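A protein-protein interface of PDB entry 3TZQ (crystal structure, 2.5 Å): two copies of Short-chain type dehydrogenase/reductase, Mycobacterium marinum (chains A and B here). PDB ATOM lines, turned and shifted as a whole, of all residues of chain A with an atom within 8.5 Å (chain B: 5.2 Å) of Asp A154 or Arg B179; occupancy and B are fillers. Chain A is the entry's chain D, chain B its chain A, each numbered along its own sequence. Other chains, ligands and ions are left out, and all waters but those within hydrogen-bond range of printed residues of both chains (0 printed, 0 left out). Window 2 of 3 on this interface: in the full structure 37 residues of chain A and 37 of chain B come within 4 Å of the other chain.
The side-chain amide nitrogen (NE2) of Gln B176 lies within hydrogen-bond range of the backbone carbonyl oxygen (O) of Tyr A153 (2.9 Å). The side-chain hydroxyl (OG1) of Thr A157 lies within hydrogen-bond range of the side-chain amide nitrogen (NE2) of Gln B176 (3.4 Å). OH of Tyr B177 sits at hydrogen-bond distance from OG1 of Thr A104, at 2.6 Å. NH2 of Arg B179 is in salt-bridge range of OD1 of Asp A154, 3.5 Å away. N of Val A103 sits at hydrogen-bond distance from OE1 of Gln B176.
The guanidinium group (NE) of Arg B179 is in hydrogen-bond range of the backbone carbonyl oxygen (O) of Gln B176 (3.0 Å). The side-chain carboxylate of Asp A100 lies within hydrogen-bond range of the backbone NH of Thr A157 (3.0 Å). The backbone carbonyl oxygen of Met A101 sits at hydrogen-bond distance from the side-chain hydroxyl of Thr A157, 2.7 Å away. OH of Tyr A153 is in hydrogen-bond range of OG of Ser A156, at 3.4 Å. The side-chain amide oxygen (OE1) of Gln A105 lies close to the backbone NH (N) of Leu A102 (3.3 Å).
CD2 of Leu A102 touches CD of Gln B176 (3.4 Å). Leu A102 touches Tyr B177 (CB to OH, 3.4 Å). Tyr B177 touches Val A103. Ala A152 touches Thr B175. Asp A154 touches Gln B176.
Of the printed residues of chain B, Val A103 touches Gln B176 (3.1 Å) and Tyr B177 (3.6 Å). Of the printed residues of chain B, Ala A152 touches Thr B175 (3.5 Å). Printed residues of chain A within 4 Å of Arg B179: Asp A154. The nearest residue of chain B that does not touch Asp A154 is Thr B175 (4.8 Å).
Of the 15 printed residues of chain A, 7 touch a printed residue of chain B. Printed residues of chain A that touch a printed residue of chain B: Leu A102, Val A103, Thr A104, Ala A152, Tyr A153, Asp A154 and Thr A157. Along chain B the printed residues that touch a printed residue of chain A span positions 175 to 179. Among the printed residues, Asp or Glu carboxylates within 4 Å of a Lys or Arg side-chain nitrogen of the other chain: Asp A154 with Arg B179.
No position is printed for both chains.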
ATOM      1  N   ALA A  99      17.900  -2.970 -10.825  1.00  0.00           N
ATOM      2  CA  ALA A  99      17.188  -3.319 -12.087  1.00  0.00           C
ATOM      3  C   ALA A  99      15.972  -2.402 -12.391  1.00  0.00           C
ATOM      4  O   ALA A  99      15.200  -2.685 -13.303  1.00  0.00           O
ATOM      5  CB  ALA A  99      16.762  -4.778 -12.063  1.00  0.00           C
ATOM      6  N   ASP A 100      15.820  -1.325 -11.610  1.00  0.00           N
ATOM      7  CA  ASP A 100      14.728  -0.372 -11.735  1.00  0.00           C
ATOM      8  C   ASP A 100      15.119   0.649 -12.795  1.00  0.00           C
ATOM      9  O   ASP A 100      15.625   1.725 -12.485  1.00  0.00           O
ATOM     10  CB  ASP A 100      14.453   0.313 -10.380  1.00  0.00           C
ATOM     11  CG  ASP A 100      13.220   1.272 -10.405  1.00  0.00           C
ATOM     12  OD1 ASP A 100      12.585   1.482 -11.461  1.00  0.00           O
ATOM     13  OD2 ASP A 100      12.885   1.833  -9.337  1.00  0.00           O
ATOM     14  N   MET A 101      14.886   0.290 -14.055  1.00  0.00           N
ATOM     15  CA  MET A 101      15.333   1.097 -15.164  1.00  0.00           C
ATOM     16  C   MET A 101      14.126   1.692 -15.937  1.00  0.00           C
ATOM     17  O   MET A 101      13.362   2.462 -15.372  1.00  0.00           O
ATOM     18  CB  MET A 101      16.288   0.261 -16.034  1.00  0.00           C
ATOM     19  CG  MET A 101      17.592  -0.136 -15.331  1.00  0.00           C
ATOM     20  SD  MET A 101      18.518   1.239 -14.565  1.00  0.00           S
ATOM     21  CE  MET A 101      19.979   0.423 -13.901  1.00  0.00           C
ATOM     22  N   LEU A 102      13.952   1.324 -17.203  1.00  0.00           N
ATOM     23  CA  LEU A 102      12.917   1.902 -18.054  1.00  0.00           C
ATOM     24  C   LEU A 102      11.557   1.233 -17.876  1.00  0.00           C
ATOM     25  O   LEU A 102      11.472   0.061 -17.489  1.00  0.00           O
ATOM     26  CB  LEU A 102      13.324   1.774 -19.516  1.00  0.00           C
ATOM     27  CG  LEU A 102      14.607   2.479 -19.896  1.00  0.00           C
ATOM     28  CD1 LEU A 102      15.199   1.856 -21.154  1.00  0.00           C
ATOM     29  CD2 LEU A 102      14.295   3.948 -20.072  1.00  0.00           C
ATOM     30  N   VAL A 103      10.500   1.987 -18.199  1.00  0.00           N
ATOM     31  CA  VAL A 103       9.134   1.475 -18.150  1.00  0.00           C
ATOM     32  C   VAL A 103       9.050   0.148 -18.867  1.00  0.00           C
ATOM     33  O   VAL A 103       8.627  -0.845 -18.286  1.00  0.00           O
ATOM     34  CB  VAL A 103       8.123   2.424 -18.799  1.00  0.00           C
ATOM     35  CG1 VAL A 103       6.746   1.780 -18.795  1.00  0.00           C
ATOM     36  CG2 VAL A 103       8.093   3.734 -18.037  1.00  0.00           C
ATOM     37  N   THR A 104       9.483   0.136 -20.127  1.00  0.00           N
ATOM     38  CA  THR A 104       9.430  -1.071 -20.955  1.00  0.00           C
ATOM     39  C   THR A 104      10.260  -2.228 -20.398  1.00  0.00           C
ATOM     40  O   THR A 104       9.979  -3.373 -20.718  1.00  0.00           O
ATOM     41  CB  THR A 104       9.909  -0.806 -22.400  1.00  0.00           C
ATOM     42  OG1 THR A 104      11.226  -0.245 -22.368  1.00  0.00           O
ATOM     43  CG2 THR A 104       8.919   0.122 -23.141  1.00  0.00           C
ATOM     44  N   GLN A 105      11.277  -1.933 -19.593  1.00  0.00           N
ATOM     45  CA  GLN A 105      12.081  -2.983 -18.954  1.00  0.00           C
ATOM     46  C   GLN A 105      11.584  -3.435 -17.565  1.00  0.00           C
ATOM     47  O   GLN A 105      12.152  -4.363 -16.979  1.00  0.00           O
ATOM     48  CB  GLN A 105      13.531  -2.517 -18.833  1.00  0.00           C
ATOM     49  CG  GLN A 105      14.274  -2.423 -20.158  1.00  0.00           C
ATOM     50  CD  GLN A 105      15.577  -1.662 -20.002  1.00  0.00           C
ATOM     51  OE1 GLN A 105      15.654  -0.689 -19.229  1.00  0.00           O
ATOM     52  NE2 GLN A 105      16.604  -2.089 -20.734  1.00  0.00           N
ATOM     53  N   ALA A 151      10.069  15.012 -11.667  1.00  0.00           N
ATOM     54  CA  ALA A 151      10.728  15.128 -12.953  1.00  0.00           C
ATOM     55  C   ALA A 151      11.539  13.853 -13.240  1.00  0.00           C
ATOM     56  O   ALA A 151      12.300  13.369 -12.400  1.00  0.00           O
ATOM     57  CB  ALA A 151      11.606  16.370 -12.989  1.00  0.00           C
ATOM     58  N   ALA A 152      11.336  13.315 -14.431  1.00  0.00           N
ATOM     59  CA  ALA A 152      11.692  11.947 -14.751  1.00  0.00           C
ATOM     60  C   ALA A 152      13.095  11.813 -15.363  1.00  0.00           C
ATOM     61  O   ALA A 152      13.688  12.792 -15.796  1.00  0.00           O
ATOM     62  CB  ALA A 152      10.628  11.369 -15.691  1.00  0.00           C
ATOM     63  N   TYR A 153      13.625  10.590 -15.372  1.00  0.00           N
ATOM     64  CA  TYR A 153      14.779  10.246 -16.218  1.00  0.00           C
ATOM     65  C   TYR A 153      14.733   8.778 -16.567  1.00  0.00           C
ATOM     66  O   TYR A 153      13.704   8.140 -16.411  1.00  0.00           O
ATOM     67  CB  TYR A 153      16.147  10.688 -15.629  1.00  0.00           C
ATOM     68  CG  TYR A 153      16.664  10.053 -14.333  1.00  0.00           C
ATOM     69  CD1 TYR A 153      18.045   9.932 -14.093  1.00  0.00           C
ATOM     70  CD2 TYR A 153      15.794   9.629 -13.325  1.00  0.00           C
ATOM     71  CE1 TYR A 153      18.530   9.394 -12.909  1.00  0.00           C
ATOM     72  CE2 TYR A 153      16.273   9.088 -12.135  1.00  0.00           C
ATOM     73  CZ  TYR A 153      17.634   8.970 -11.924  1.00  0.00           C
ATOM     74  OH  TYR A 153      18.060   8.422 -10.710  1.00  0.00           O
ATOM     75  N   ASP A 154      15.839   8.244 -17.065  1.00  0.00           N
ATOM     76  CA  ASP A 154      15.826   6.912 -17.660  1.00  0.00           C
ATOM     77  C   ASP A 154      16.023   5.816 -16.641  1.00  0.00           C
ATOM     78  O   ASP A 154      16.340   4.699 -17.009  1.00  0.00           O
ATOM     79  CB  ASP A 154      16.856   6.813 -18.795  1.00  0.00           C
ATOM     80  CG  ASP A 154      16.592   7.831 -19.887  1.00  0.00           C
ATOM     81  OD1 ASP A 154      15.392   8.102 -20.147  1.00  0.00           O
ATOM     82  OD2 ASP A 154      17.556   8.372 -20.476  1.00  0.00           O
ATOM     83  N   MET A 155      15.833   6.125 -15.363  1.00  0.00           N
ATOM     84  CA  MET A 155      15.961   5.102 -14.334  1.00  0.00           C
ATOM     85  C   MET A 155      15.140   5.492 -13.114  1.00  0.00           C
ATOM     86  O   MET A 155      14.749   6.652 -12.962  1.00  0.00           O
ATOM     87  CB  MET A 155      17.441   4.792 -13.998  1.00  0.00           C
ATOM     88  CG  MET A 155      18.144   5.764 -13.048  1.00  0.00           C
ATOM     89  SD  MET A 155      19.839   5.268 -12.599  1.00  0.00           S
ATOM     90  CE  MET A 155      20.603   5.436 -14.220  1.00  0.00           C
ATOM     91  N   SER A 156      14.849   4.495 -12.286  1.00  0.00           N
ATOM     92  CA  SER A 156      14.206   4.678 -10.982  1.00  0.00           C
ATOM     93  C   SER A 156      12.715   4.970 -11.104  1.00  0.00           C
ATOM     94  O   SER A 156      12.166   5.719 -10.303  1.00  0.00           O
ATOM     95  CB  SER A 156      14.896   5.785 -10.172  1.00  0.00           C
ATOM     96  OG  SER A 156      16.295   5.616 -10.184  1.00  0.00           O
ATOM     97  N   THR A 157      12.071   4.365 -12.106  1.00  0.00           N
ATOM     98  CA  THR A 157      10.677   4.634 -12.408  1.00  0.00           C
ATOM     99  C   THR A 157       9.775   4.193 -11.254  1.00  0.00           C
ATOM    100  O   THR A 157       8.957   4.984 -10.746  1.00  0.00           O
ATOM    101  CB  THR A 157      10.234   3.923 -13.699  1.00  0.00           C
ATOM    102  OG1 THR A 157      11.290   3.969 -14.656  1.00  0.00           O
ATOM    103  CG2 THR A 157       9.001   4.605 -14.283  1.00  0.00           C
ATOM    104  N   PHE A 209      24.654  16.235 -12.768  1.00  0.00           N
ATOM    105  CA  PHE A 209      23.647  16.624 -11.793  1.00  0.00           C
ATOM    106  C   PHE A 209      24.066  17.776 -10.888  1.00  0.00           C
ATOM    107  O   PHE A 209      23.272  18.691 -10.649  1.00  0.00           O
ATOM    108  CB  PHE A 209      23.288  15.445 -10.909  1.00  0.00           C
ATOM    109  CG  PHE A 209      22.351  14.477 -11.547  1.00  0.00           C
ATOM    110  CD1 PHE A 209      21.169  14.908 -12.121  1.00  0.00           C
ATOM    111  CD2 PHE A 209      22.623  13.137 -11.538  1.00  0.00           C
ATOM    112  CE1 PHE A 209      20.280  14.013 -12.704  1.00  0.00           C
ATOM    113  CE2 PHE A 209      21.724  12.240 -12.094  1.00  0.00           C
ATOM    114  CZ  PHE A 209      20.551  12.681 -12.673  1.00  0.00           C
ATOM    115  N   THR B 175       9.140  11.145 -20.856  1.00  0.00           N
ATOM    116  CA  THR B 175      10.565  11.475 -20.881  1.00  0.00           C
ATOM    117  C   THR B 175      11.411  10.409 -21.602  1.00  0.00           C
ATOM    118  O   THR B 175      12.163  10.714 -22.544  1.00  0.00           O
ATOM    119  CB  THR B 175      11.086  11.700 -19.446  1.00  0.00           C
ATOM    120  OG1 THR B 175      10.459  12.863 -18.904  1.00  0.00           O
ATOM    121  CG2 THR B 175      12.612  11.899 -19.409  1.00  0.00           C
ATOM    122  N   GLN B 176      11.282   9.161 -21.159  1.00  0.00           N
ATOM    123  CA  GLN B 176      12.048   8.032 -21.728  1.00  0.00           C
ATOM    124  C   GLN B 176      11.768   7.745 -23.234  1.00  0.00           C
ATOM    125  O   GLN B 176      12.654   7.264 -23.962  1.00  0.00           O
ATOM    126  CB  GLN B 176      11.781   6.765 -20.913  1.00  0.00           C
ATOM    127  CG  GLN B 176      12.308   6.872 -19.494  1.00  0.00           C
ATOM    128  CD  GLN B 176      11.810   5.771 -18.585  1.00  0.00           C
ATOM    129  OE1 GLN B 176      11.047   4.883 -18.994  1.00  0.00           O
ATOM    130  NE2 GLN B 176      12.262   5.812 -17.329  1.00  0.00           N
ATOM    131  N   TYR B 177      10.548   8.040 -23.689  1.00  0.00           N
ATOM    132  CA  TYR B 177      10.135   7.645 -25.035  1.00  0.00           C
ATOM    133  C   TYR B 177       9.786   8.826 -25.964  1.00  0.00           C
ATOM    134  O   TYR B 177       9.486   8.638 -27.144  1.00  0.00           O
ATOM    135  CB  TYR B 177       9.039   6.582 -24.940  1.00  0.00           C
ATOM    136  CG  TYR B 177       9.494   5.399 -24.090  1.00  0.00           C
ATOM    137  CD1 TYR B 177      10.318   4.413 -24.621  1.00  0.00           C
ATOM    138  CD2 TYR B 177       9.143   5.304 -22.745  1.00  0.00           C
ATOM    139  CE1 TYR B 177      10.751   3.342 -23.852  1.00  0.00           C
ATOM    140  CE2 TYR B 177       9.599   4.258 -21.952  1.00  0.00           C
ATOM    141  CZ  TYR B 177      10.401   3.275 -22.511  1.00  0.00           C
ATOM    142  OH  TYR B 177      10.841   2.212 -21.742  1.00  0.00           O
ATOM    143  N   GLY B 178       9.896  10.046 -25.452  1.00  0.00           N
ATOM    144  CA  GLY B 178       9.750  11.215 -26.302  1.00  0.00           C
ATOM    145  C   GLY B 178      10.635  11.104 -27.530  1.00  0.00           C
ATOM    146  O   GLY B 178      10.190  11.272 -28.669  1.00  0.00           O
ATOM    147  N   ARG B 179      11.889  10.770 -27.304  1.00  0.00           N
ATOM    148  CA  ARG B 179      12.827  10.634 -28.407  1.00  0.00           C
ATOM    149  C   ARG B 179      12.331   9.634 -29.476  1.00  0.00           C
ATOM    150  O   ARG B 179      12.645   9.791 -30.651  1.00  0.00           O
ATOM    151  CB  ARG B 179      14.234  10.277 -27.890  1.00  0.00           C
ATOM    152  CG  ARG B 179      14.333   8.906 -27.248  1.00  0.00           C
ATOM    153  CD  ARG B 179      15.626   8.664 -26.447  1.00  0.00           C
ATOM    154  NE  ARG B 179      15.333   7.900 -25.201  1.00  0.00           N
ATOM    155  CZ  ARG B 179      16.239   7.299 -24.416  1.00  0.00           C
ATOM    156  NH1 ARG B 179      17.549   7.352 -24.710  1.00  0.00           N
ATOM    157  NH2 ARG B 179      15.828   6.637 -23.332  1.00  0.00           N
ATOM    158  N   HIS B 180      11.553   8.626 -29.080  1.00  0.00           N
ATOM    159  CA  HIS B 180      10.991   7.682 -30.057  1.00  0.00           C
ATOM    160  C   HIS B 180       9.620   8.031 -30.577  1.00  0.00           C
ATOM    161  O   HIS B 180       9.027   7.252 -31.327  1.00  0.00           O
ATOM    162  CB  HIS B 180      10.998   6.283 -29.477  1.00  0.00           C
ATOM    163  CG  HIS B 180      12.361   5.853 -29.001  1.00  0.00           C
ATOM    164  ND1 HIS B 180      13.398   5.679 -29.850  1.00  0.00           N
ATOM    165  CD2 HIS B 180      12.857   5.640 -27.710  1.00  0.00           C
ATOM    166  CE1 HIS B 180      14.478   5.331 -29.143  1.00  0.00           C
ATOM    167  NE2 HIS B 180      14.141   5.311 -27.830  1.00  0.00           N
ATOM    168  N   GLY B 181       9.110   9.208 -30.217  1.00  0.00           N
ATOM    169  CA  GLY B 181       7.863   9.709 -30.789  1.00  0.00           C
ATOM    170  C   GLY B 181       6.598   9.398 -29.997  1.00  0.00           C
ATOM    171  O   GLY B 181       5.495   9.517 -30.525  1.00  0.00           O
